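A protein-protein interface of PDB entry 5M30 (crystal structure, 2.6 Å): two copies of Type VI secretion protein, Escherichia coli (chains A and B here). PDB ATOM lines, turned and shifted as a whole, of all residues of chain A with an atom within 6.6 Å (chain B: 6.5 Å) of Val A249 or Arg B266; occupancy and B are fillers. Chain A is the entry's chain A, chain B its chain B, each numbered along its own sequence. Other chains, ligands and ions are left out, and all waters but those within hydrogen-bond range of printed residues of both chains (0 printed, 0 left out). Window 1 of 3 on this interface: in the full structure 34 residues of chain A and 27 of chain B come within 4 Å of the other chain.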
ATOM      1  N   ASN A 244      14.956  17.775  33.701  1.00  0.00           N
ATOM      2  CA  ASN A 244      13.852  18.687  33.416  1.00  0.00           C
ATOM      3  C   ASN A 244      14.088  19.542  32.181  1.00  0.00           C
ATOM      4  O   ASN A 244      13.120  19.941  31.539  1.00  0.00           O
ATOM      5  CB  ASN A 244      13.499  19.534  34.630  1.00  0.00           C
ATOM      6  CG  ASN A 244      12.886  18.748  35.771  1.00  0.00           C
ATOM      7  OD1 ASN A 244      13.477  18.607  36.823  1.00  0.00           O
ATOM      8  ND2 ASN A 244      11.678  18.219  35.599  1.00  0.00           N
ATOM      9  N   SER A 245      15.362  19.810  31.841  1.00  0.00           N
ATOM     10  CA  SER A 245      15.728  20.571  30.655  1.00  0.00           C
ATOM     11  C   SER A 245      15.490  19.737  29.400  1.00  0.00           C
ATOM     12  O   SER A 245      14.973  20.255  28.418  1.00  0.00           O
ATOM     13  CB  SER A 245      17.200  20.966  30.700  1.00  0.00           C
ATOM     14  OG  SER A 245      17.442  21.929  31.706  1.00  0.00           O
ATOM     15  N   ALA A 246      15.877  18.463  29.434  1.00  0.00           N
ATOM     16  CA  ALA A 246      15.799  17.519  28.340  1.00  0.00           C
ATOM     17  C   ALA A 246      14.413  16.979  28.040  1.00  0.00           C
ATOM     18  O   ALA A 246      14.079  16.817  26.871  1.00  0.00           O
ATOM     19  CB  ALA A 246      16.743  16.369  28.604  1.00  0.00           C
ATOM     20  N   GLU A 247      13.641  16.617  29.077  1.00  0.00           N
ATOM     21  CA  GLU A 247      12.329  15.989  28.934  1.00  0.00           C
ATOM     22  C   GLU A 247      11.418  16.708  27.917  1.00  0.00           C
ATOM     23  O   GLU A 247      11.058  16.075  26.919  1.00  0.00           O
ATOM     24  CB  GLU A 247      11.648  15.807  30.305  1.00  0.00           C
ATOM     25  CG  GLU A 247      10.620  14.682  30.373  1.00  0.00           C
ATOM     26  CD  GLU A 247       9.209  14.936  29.865  1.00  0.00           C
ATOM     27  OE1 GLU A 247       8.805  16.114  29.710  1.00  0.00           O
ATOM     28  OE2 GLU A 247       8.515  13.933  29.590  1.00  0.00           O
ATOM     29  N   PRO A 248      11.068  18.012  28.076  1.00  0.00           N
ATOM     30  CA  PRO A 248      10.183  18.642  27.073  1.00  0.00           C
ATOM     31  C   PRO A 248      10.720  18.621  25.636  1.00  0.00           C
ATOM     32  O   PRO A 248       9.944  18.434  24.697  1.00  0.00           O
ATOM     33  CB  PRO A 248       9.978  20.062  27.610  1.00  0.00           C
ATOM     34  CG  PRO A 248      11.105  20.297  28.556  1.00  0.00           C
ATOM     35  CD  PRO A 248      11.401  18.961  29.161  1.00  0.00           C
ATOM     36  N   VAL A 249      12.044  18.771  25.475  1.00  0.00           N
ATOM     37  CA  VAL A 249      12.722  18.790  24.182  1.00  0.00           C
ATOM     38  C   VAL A 249      12.713  17.399  23.530  1.00  0.00           C
ATOM     39  O   VAL A 249      12.343  17.289  22.372  1.00  0.00           O
ATOM     40  CB  VAL A 249      14.124  19.432  24.299  1.00  0.00           C
ATOM     41  CG1 VAL A 249      14.876  19.347  22.983  1.00  0.00           C
ATOM     42  CG2 VAL A 249      14.005  20.894  24.743  1.00  0.00           C
ATOM     43  N   LEU A 250      13.031  16.345  24.273  1.00  0.00           N
ATOM     44  CA  LEU A 250      13.010  15.000  23.710  1.00  0.00           C
ATOM     45  C   LEU A 250      11.605  14.490  23.443  1.00  0.00           C
ATOM     46  O   LEU A 250      11.411  13.687  22.537  1.00  0.00           O
ATOM     47  CB  LEU A 250      13.798  14.007  24.585  1.00  0.00           C
ATOM     48  CG  LEU A 250      15.268  14.353  24.879  1.00  0.00           C
ATOM     49  CD1 LEU A 250      15.813  13.523  26.051  1.00  0.00           C
ATOM     50  CD2 LEU A 250      16.148  14.239  23.617  1.00  0.00           C
ATOM     51  N   LYS A 251      10.631  14.945  24.233  1.00  0.00           N
ATOM     52  CA  LYS A 251       9.234  14.567  24.093  1.00  0.00           C
ATOM     53  C   LYS A 251       8.706  15.072  22.758  1.00  0.00           C
ATOM     54  O   LYS A 251       8.076  14.282  22.056  1.00  0.00           O
ATOM     55  CB  LYS A 251       8.400  15.135  25.263  1.00  0.00           C
ATOM     56  CG  LYS A 251       7.423  14.134  25.868  1.00  0.00           C
ATOM     57  CD  LYS A 251       6.704  14.682  27.080  1.00  0.00           C
ATOM     58  N   GLU A 252       8.999  16.365  22.378  1.00  0.00           N
ATOM     59  CA  GLU A 252       8.524  16.956  21.113  1.00  0.00           C
ATOM     60  C   GLU A 252       9.219  16.318  19.888  1.00  0.00           C
ATOM     61  O   GLU A 252       8.577  16.160  18.849  1.00  0.00           O
ATOM     62  CB  GLU A 252       8.576  18.512  21.098  1.00  0.00           C
ATOM     63  CG  GLU A 252       9.668  19.166  20.244  1.00  0.00           C
ATOM     64  CD  GLU A 252       9.376  19.434  18.777  1.00  0.00           C
ATOM     65  OE1 GLU A 252       8.261  19.106  18.305  1.00  0.00           O
ATOM     66  OE2 GLU A 252      10.273  19.989  18.100  1.00  0.00           O
ATOM     67  N   LEU A 253      10.503  15.920  20.029  1.00  0.00           N
ATOM     68  CA  LEU A 253      11.256  15.282  18.963  1.00  0.00           C
ATOM     69  C   LEU A 253      10.725  13.903  18.705  1.00  0.00           C
ATOM     70  O   LEU A 253      10.832  13.417  17.578  1.00  0.00           O
ATOM     71  CB  LEU A 253      12.766  15.238  19.256  1.00  0.00           C
ATOM     72  CG  LEU A 253      13.492  16.578  19.204  1.00  0.00           C
ATOM     73  CD1 LEU A 253      14.912  16.455  19.709  1.00  0.00           C
ATOM     74  CD2 LEU A 253      13.448  17.183  17.834  1.00  0.00           C
ATOM     75  N   LEU A 254      10.121  13.281  19.719  1.00  0.00           N
ATOM     76  CA  LEU A 254       9.550  11.948  19.597  1.00  0.00           C
ATOM     77  C   LEU A 254       8.041  11.918  19.260  1.00  0.00           C
ATOM     78  O   LEU A 254       7.588  10.924  18.682  1.00  0.00           O
ATOM     79  CB  LEU A 254       9.858  11.130  20.834  1.00  0.00           C
ATOM     80  CG  LEU A 254      10.850  10.041  20.557  1.00  0.00           C
ATOM     81  CD1 LEU A 254      12.069  10.198  21.438  1.00  0.00           C
ATOM     82  CD2 LEU A 254      10.174   8.659  20.637  1.00  0.00           C
ATOM     83  N   ARG A 259      11.644  14.159  11.455  1.00  0.00           N
ATOM     84  CA  ARG A 259      12.761  15.064  11.201  1.00  0.00           C
ATOM     85  C   ARG A 259      14.025  14.269  11.161  1.00  0.00           C
ATOM     86  O   ARG A 259      14.034  13.109  11.560  1.00  0.00           O
ATOM     87  CB  ARG A 259      12.855  16.154  12.263  1.00  0.00           C
ATOM     88  CG  ARG A 259      11.801  17.217  12.145  1.00  0.00           C
ATOM     89  CD  ARG A 259      11.853  18.031  13.381  1.00  0.00           C
ATOM     90  NE  ARG A 259      10.771  17.887  14.368  1.00  0.00           N
ATOM     91  CZ  ARG A 259      10.698  16.940  15.276  1.00  0.00           C
ATOM     92  NH1 ARG A 259      11.535  15.903  15.235  1.00  0.00           N
ATOM     93  NH2 ARG A 259       9.714  16.941  16.165  1.00  0.00           N
ATOM     94  N   LEU A 263      19.134  16.189  14.737  1.00  0.00           N
ATOM     95  CA  LEU A 263      18.421  16.986  15.739  1.00  0.00           C
ATOM     96  C   LEU A 263      18.319  16.199  17.028  1.00  0.00           C
ATOM     97  O   LEU A 263      18.578  16.751  18.091  1.00  0.00           O
ATOM     98  CB  LEU A 263      16.991  17.267  15.270  1.00  0.00           C
ATOM     99  CG  LEU A 263      16.694  18.644  14.769  1.00  0.00           C
ATOM    100  CD1 LEU A 263      16.918  18.720  13.179  1.00  0.00           C
ATOM    101  CD2 LEU A 263      15.274  19.049  15.202  1.00  0.00           C
ATOM    102  N   GLU A 267      20.461  16.590  20.922  1.00  0.00           N
ATOM    103  CA  GLU A 267      19.765  16.735  22.192  1.00  0.00           C
ATOM    104  C   GLU A 267      19.976  15.544  23.124  1.00  0.00           C
ATOM    105  O   GLU A 267      19.999  15.717  24.344  1.00  0.00           O
ATOM    106  CB  GLU A 267      18.284  17.055  21.959  1.00  0.00           C
ATOM    107  CG  GLU A 267      18.068  18.444  21.358  1.00  0.00           C
ATOM    108  CD  GLU A 267      18.511  19.645  22.182  1.00  0.00           C
ATOM    109  OE1 GLU A 267      18.586  19.527  23.429  1.00  0.00           O
ATOM    110  OE2 GLU A 267      18.743  20.720  21.580  1.00  0.00           O
ATOM    111  N   ARG A 270      23.589  16.052  24.293  1.00  0.00           N
ATOM    112  CA  ARG A 270      23.586  17.164  25.248  1.00  0.00           C
ATOM    113  C   ARG A 270      23.216  16.633  26.652  1.00  0.00           C
ATOM    114  O   ARG A 270      23.772  17.090  27.654  1.00  0.00           O
ATOM    115  CB  ARG A 270      22.568  18.225  24.812  1.00  0.00           C
ATOM    116  CG  ARG A 270      22.709  19.537  25.568  1.00  0.00           C
ATOM    117  CD  ARG A 270      21.533  20.499  25.423  1.00  0.00           C
ATOM    118  NE  ARG A 270      21.187  20.808  24.033  1.00  0.00           N
ATOM    119  CZ  ARG A 270      21.840  21.671  23.248  1.00  0.00           C
ATOM    120  NH1 ARG A 270      22.912  22.311  23.696  1.00  0.00           N
ATOM    121  NH2 ARG A 270      21.438  21.878  21.999  1.00  0.00           N
ATOM    122  N   GLY B  37      13.810  19.356   8.944  1.00  0.00           N
ATOM    123  CA  GLY B  37      14.102  20.209  10.085  1.00  0.00           C
ATOM    124  C   GLY B  37      12.883  20.643  10.859  1.00  0.00           C
ATOM    125  O   GLY B  37      13.018  21.107  11.993  1.00  0.00           O
ATOM    126  N   LEU B  38      11.685  20.515  10.266  1.00  0.00           N
ATOM    127  CA  LEU B  38      10.447  20.968  10.904  1.00  0.00           C
ATOM    128  C   LEU B  38       9.365  19.926  10.785  1.00  0.00           C
ATOM    129  O   LEU B  38       9.211  19.349   9.701  1.00  0.00           O
ATOM    130  CB  LEU B  38       9.957  22.277  10.242  1.00  0.00           C
ATOM    131  CG  LEU B  38      10.885  23.494  10.217  1.00  0.00           C
ATOM    132  CD1 LEU B  38      10.330  24.519   9.300  1.00  0.00           C
ATOM    133  CD2 LEU B  38      11.091  24.077  11.607  1.00  0.00           C
ATOM    134  N   PRO B 261       8.037  28.802  14.586  1.00  0.00           N
ATOM    135  CA  PRO B 261       7.945  28.798  16.058  1.00  0.00           C
ATOM    136  C   PRO B 261       8.387  27.533  16.792  1.00  0.00           C
ATOM    137  O   PRO B 261       8.485  27.568  18.009  1.00  0.00           O
ATOM    138  CB  PRO B 261       6.460  29.078  16.314  1.00  0.00           C
ATOM    139  CG  PRO B 261       5.964  29.683  15.080  1.00  0.00           C
ATOM    140  CD  PRO B 261       6.712  29.042  13.986  1.00  0.00           C
ATOM    141  N   GLU B 262       8.633  26.434  16.080  1.00  0.00           N
ATOM    142  CA  GLU B 262       9.123  25.174  16.653  1.00  0.00           C
ATOM    143  C   GLU B 262      10.486  25.390  17.328  1.00  0.00           C
ATOM    144  O   GLU B 262      10.821  24.691  18.285  1.00  0.00           O
ATOM    145  CB  GLU B 262       9.315  24.123  15.547  1.00  0.00           C
ATOM    146  CG  GLU B 262       8.136  23.199  15.335  1.00  0.00           C
ATOM    147  CD  GLU B 262       8.379  22.162  14.267  1.00  0.00           C
ATOM    148  OE1 GLU B 262       9.475  21.553  14.257  1.00  0.00           O
ATOM    149  OE2 GLU B 262       7.459  21.950  13.445  1.00  0.00           O
ATOM    150  N   LEU B 263      11.285  26.322  16.786  1.00  0.00           N
ATOM    151  CA  LEU B 263      12.595  26.705  17.280  1.00  0.00           C
ATOM    152  C   LEU B 263      12.451  27.402  18.610  1.00  0.00           C
ATOM    153  O   LEU B 263      13.168  27.072  19.548  1.00  0.00           O
ATOM    154  CB  LEU B 263      13.218  27.685  16.296  1.00  0.00           C
ATOM    155  CG  LEU B 263      14.294  27.160  15.385  1.00  0.00           C
ATOM    156  CD1 LEU B 263      13.687  26.624  14.026  1.00  0.00           C
ATOM    157  CD2 LEU B 263      15.335  28.238  15.143  1.00  0.00           C
ATOM    158  N   LEU B 264      11.539  28.387  18.676  1.00  0.00           N
ATOM    159  CA  LEU B 264      11.238  29.186  19.845  1.00  0.00           C
ATOM    160  C   LEU B 264      10.630  28.336  20.933  1.00  0.00           C
ATOM    161  O   LEU B 264      11.039  28.469  22.079  1.00  0.00           O
ATOM    162  CB  LEU B 264      10.295  30.339  19.488  1.00  0.00           C
ATOM    163  CG  LEU B 264       9.906  31.295  20.636  1.00  0.00           C
ATOM    164  CD1 LEU B 264      11.089  32.174  21.081  1.00  0.00           C
ATOM    165  CD2 LEU B 264       8.695  32.098  20.275  1.00  0.00           C
ATOM    166  N   TYR B 265       9.675  27.462  20.586  1.00  0.00           N
ATOM    167  CA  TYR B 265       9.050  26.565  21.538  1.00  0.00           C
ATOM    168  C   TYR B 265      10.094  25.700  22.228  1.00  0.00           C
ATOM    169  O   TYR B 265      10.109  25.639  23.452  1.00  0.00           O
ATOM    170  CB  TYR B 265       7.983  25.681  20.865  1.00  0.00           C
ATOM    171  CG  TYR B 265       7.509  24.566  21.776  1.00  0.00           C
ATOM    172  CD1 TYR B 265       6.491  24.782  22.708  1.00  0.00           C
ATOM    173  CD2 TYR B 265       8.126  23.318  21.758  1.00  0.00           C
ATOM    174  CE1 TYR B 265       6.096  23.778  23.589  1.00  0.00           C
ATOM    175  CE2 TYR B 265       7.751  22.314  22.645  1.00  0.00           C
ATOM    176  CZ  TYR B 265       6.731  22.545  23.554  1.00  0.00           C
ATOM    177  OH  TYR B 265       6.377  21.534  24.410  1.00  0.00           O
ATOM    178  N   ARG B 266      10.968  25.035  21.459  1.00  0.00           N
ATOM    179  CA  ARG B 266      12.010  24.163  22.015  1.00  0.00           C
ATOM    180  C   ARG B 266      12.854  24.851  23.087  1.00  0.00           C
ATOM    181  O   ARG B 266      13.165  24.244  24.107  1.00  0.00           O
ATOM    182  CB  ARG B 266      12.914  23.628  20.901  1.00  0.00           C
ATOM    183  CG  ARG B 266      13.915  22.581  21.369  1.00  0.00           C
ATOM    184  CD  ARG B 266      14.913  22.056  20.331  1.00  0.00           C
ATOM    185  NE  ARG B 266      14.500  22.237  18.940  1.00  0.00           N
ATOM    186  CZ  ARG B 266      13.598  21.490  18.318  1.00  0.00           C
ATOM    187  NH1 ARG B 266      12.973  20.510  18.967  1.00  0.00           N
ATOM    188  NH2 ARG B 266      13.277  21.742  17.064  1.00  0.00           N
ATOM    189  N   GLU B 267      13.227  26.105  22.848  1.00  0.00           N
ATOM    190  CA  GLU B 267      14.093  26.866  23.740  1.00  0.00           C
ATOM    191  C   GLU B 267      13.337  27.462  24.916  1.00  0.00           C
ATOM    192  O   GLU B 267      13.897  27.600  26.000  1.00  0.00           O
ATOM    193  CB  GLU B 267      14.901  27.916  22.944  1.00  0.00           C
ATOM    194  CG  GLU B 267      15.947  27.276  22.026  1.00  0.00           C
ATOM    195  CD  GLU B 267      17.048  26.451  22.673  1.00  0.00           C
ATOM    196  OE1 GLU B 267      17.366  26.686  23.860  1.00  0.00           O
ATOM    197  OE2 GLU B 267      17.630  25.596  21.969  1.00  0.00           O
ATOM    198  N   LEU B 268      12.059  27.753  24.722  1.00  0.00           N
ATOM    199  CA  LEU B 268      11.142  28.270  25.727  1.00  0.00           C
ATOM    200  C   LEU B 268      10.832  27.125  26.694  1.00  0.00           C
ATOM    201  O   LEU B 268      10.955  27.303  27.893  1.00  0.00           O
ATOM    202  CB  LEU B 268       9.863  28.742  25.003  1.00  0.00           C
ATOM    203  CG  LEU B 268       9.383  30.191  25.130  1.00  0.00           C
ATOM    204  CD1 LEU B 268      10.495  31.193  25.058  1.00  0.00           C
ATOM    205  CD2 LEU B 268       8.354  30.491  24.090  1.00  0.00           C
ATOM    206  N   ALA B 269      10.489  25.931  26.169  1.00  0.00           N
ATOM    207  CA  ALA B 269      10.211  24.728  26.957  1.00  0.00           C
ATOM    208  C   ALA B 269      11.462  24.258  27.719  1.00  0.00           C
ATOM    209  O   ALA B 269      11.336  23.797  28.859  1.00  0.00           O
ATOM    210  CB  ALA B 269       9.695  23.616  26.062  1.00  0.00           C
ATOM    211  N   ARG B 270      12.667  24.400  27.111  1.00  0.00           N
ATOM    212  CA  ARG B 270      13.935  24.045  27.745  1.00  0.00           C
ATOM    213  C   ARG B 270      14.142  24.909  29.008  1.00  0.00           C
ATOM    214  O   ARG B 270      14.639  24.426  30.019  1.00  0.00           O
ATOM    215  CB  ARG B 270      15.099  24.280  26.773  1.00  0.00           C
ATOM    216  CG  ARG B 270      16.384  23.600  27.224  1.00  0.00           C
ATOM    217  CD  ARG B 270      17.622  24.084  26.508  1.00  0.00           C
ATOM    218  NE  ARG B 270      17.526  23.953  25.051  1.00  0.00           N
ATOM    219  CZ  ARG B 270      17.754  22.839  24.373  1.00  0.00           C
ATOM    220  NH1 ARG B 270      18.112  21.732  25.008  1.00  0.00           N
ATOM    221  NH2 ARG B 270      17.649  22.827  23.048  1.00  0.00           N
ATOM    222  N   LEU B 271      13.758  26.179  28.933  1.00  0.00           N
ATOM    223  CA  LEU B 271      13.872  27.139  30.029  1.00  0.00           C
ATOM    224  C   LEU B 271      12.847  26.851  31.123  1.00  0.00           C
ATOM    225  O   LEU B 271      13.209  26.829  32.291  1.00  0.00           O
ATOM    226  CB  LEU B 271      13.729  28.570  29.488  1.00  0.00           C
ATOM    227  CG  LEU B 271      13.733  29.679  30.498  1.00  0.00           C
ATOM    228  CD1 LEU B 271      15.065  29.745  31.255  1.00  0.00           C
ATOM    229  CD2 LEU B 271      13.337  30.982  29.861  1.00  0.00           C
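NE of Arg A270 lies close to NH1 of Arg B270, at 3.4 Å. The guanidinium group of Arg B266 lies within salt-bridge range of the side-chain carboxylate of Glu A252. OE1 of Glu A267 lies within salt-bridge range of NH1 of Arg B270 (2.8 Å). NE of Arg A259 is in salt-bridge range of OE1 of Glu B262 (3.9 Å).
Of the printed residues of chain B, Val A249 touches Arg B266 (3.5 Å). Arg B266 touches four residues of chain A. Printed residues of chain B within 4 Å of Glu A267: Arg B270 (2.8 Å). Of the printed residues of chain A, Glu B262 touches Arg A259 (3.9 Å). Of the printed residues of chain A, Arg B270 touches Ser A245, Glu A267 and Arg A270. Printed residues of chain B within 4 Å of Pro A248: Ala B269. Lys A251 touches none of the printed residues of chain B. Pro B261 touches none of the printed residues of chain A. The nearest residue of chain A that does not touch Arg B266 is Glu A267 (4.2 Å). The nearest printed residue of chain A that does not touch Glu B262 is Glu A252 (4.2 Å).
Among the printed residues, pairs that only touch across the chains: Ser A245 with Arg B270 (3.8 Å), Pro A248 with Ala B269 (3.5 Å), Val A249 with Arg B266 (3.5 Å), Leu A253 with Arg B266 (3.5 Å), Arg A259 with Gly B37 (3.6 Å), Arg A259 with Leu B38 (3.8 Å) and Leu A263 with Arg B266 (3.8 Å).
Hydrophobic or aromatic side chains of chain B within 4 Å of the printed part of chain A: Ala B269. Along chain B the printed residues that touch a printed residue of chain A span positions 37 to 270.
O of Leu A253 sits close to NH1 of Arg A259 (3.5 Å). The guanidinium group of Arg B270 lies within salt-bridge range of the side-chain carboxylate of Glu B267. OE1 of Glu A252 is in salt-bridge range of NH2 of Arg A259, 3.4 Å away. The side-chain carboxylate of Glu A267 lies within salt-bridge range of the guanidinium group of Arg A270 (3.0 Å).
Glu A267 touches Arg B270, but with the chains exchanged Arg A270 does not touch Glu B267 (5.3 Å). Arg B270 touches its own counterpart, Arg A270. 3 positions are printed for both chains.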
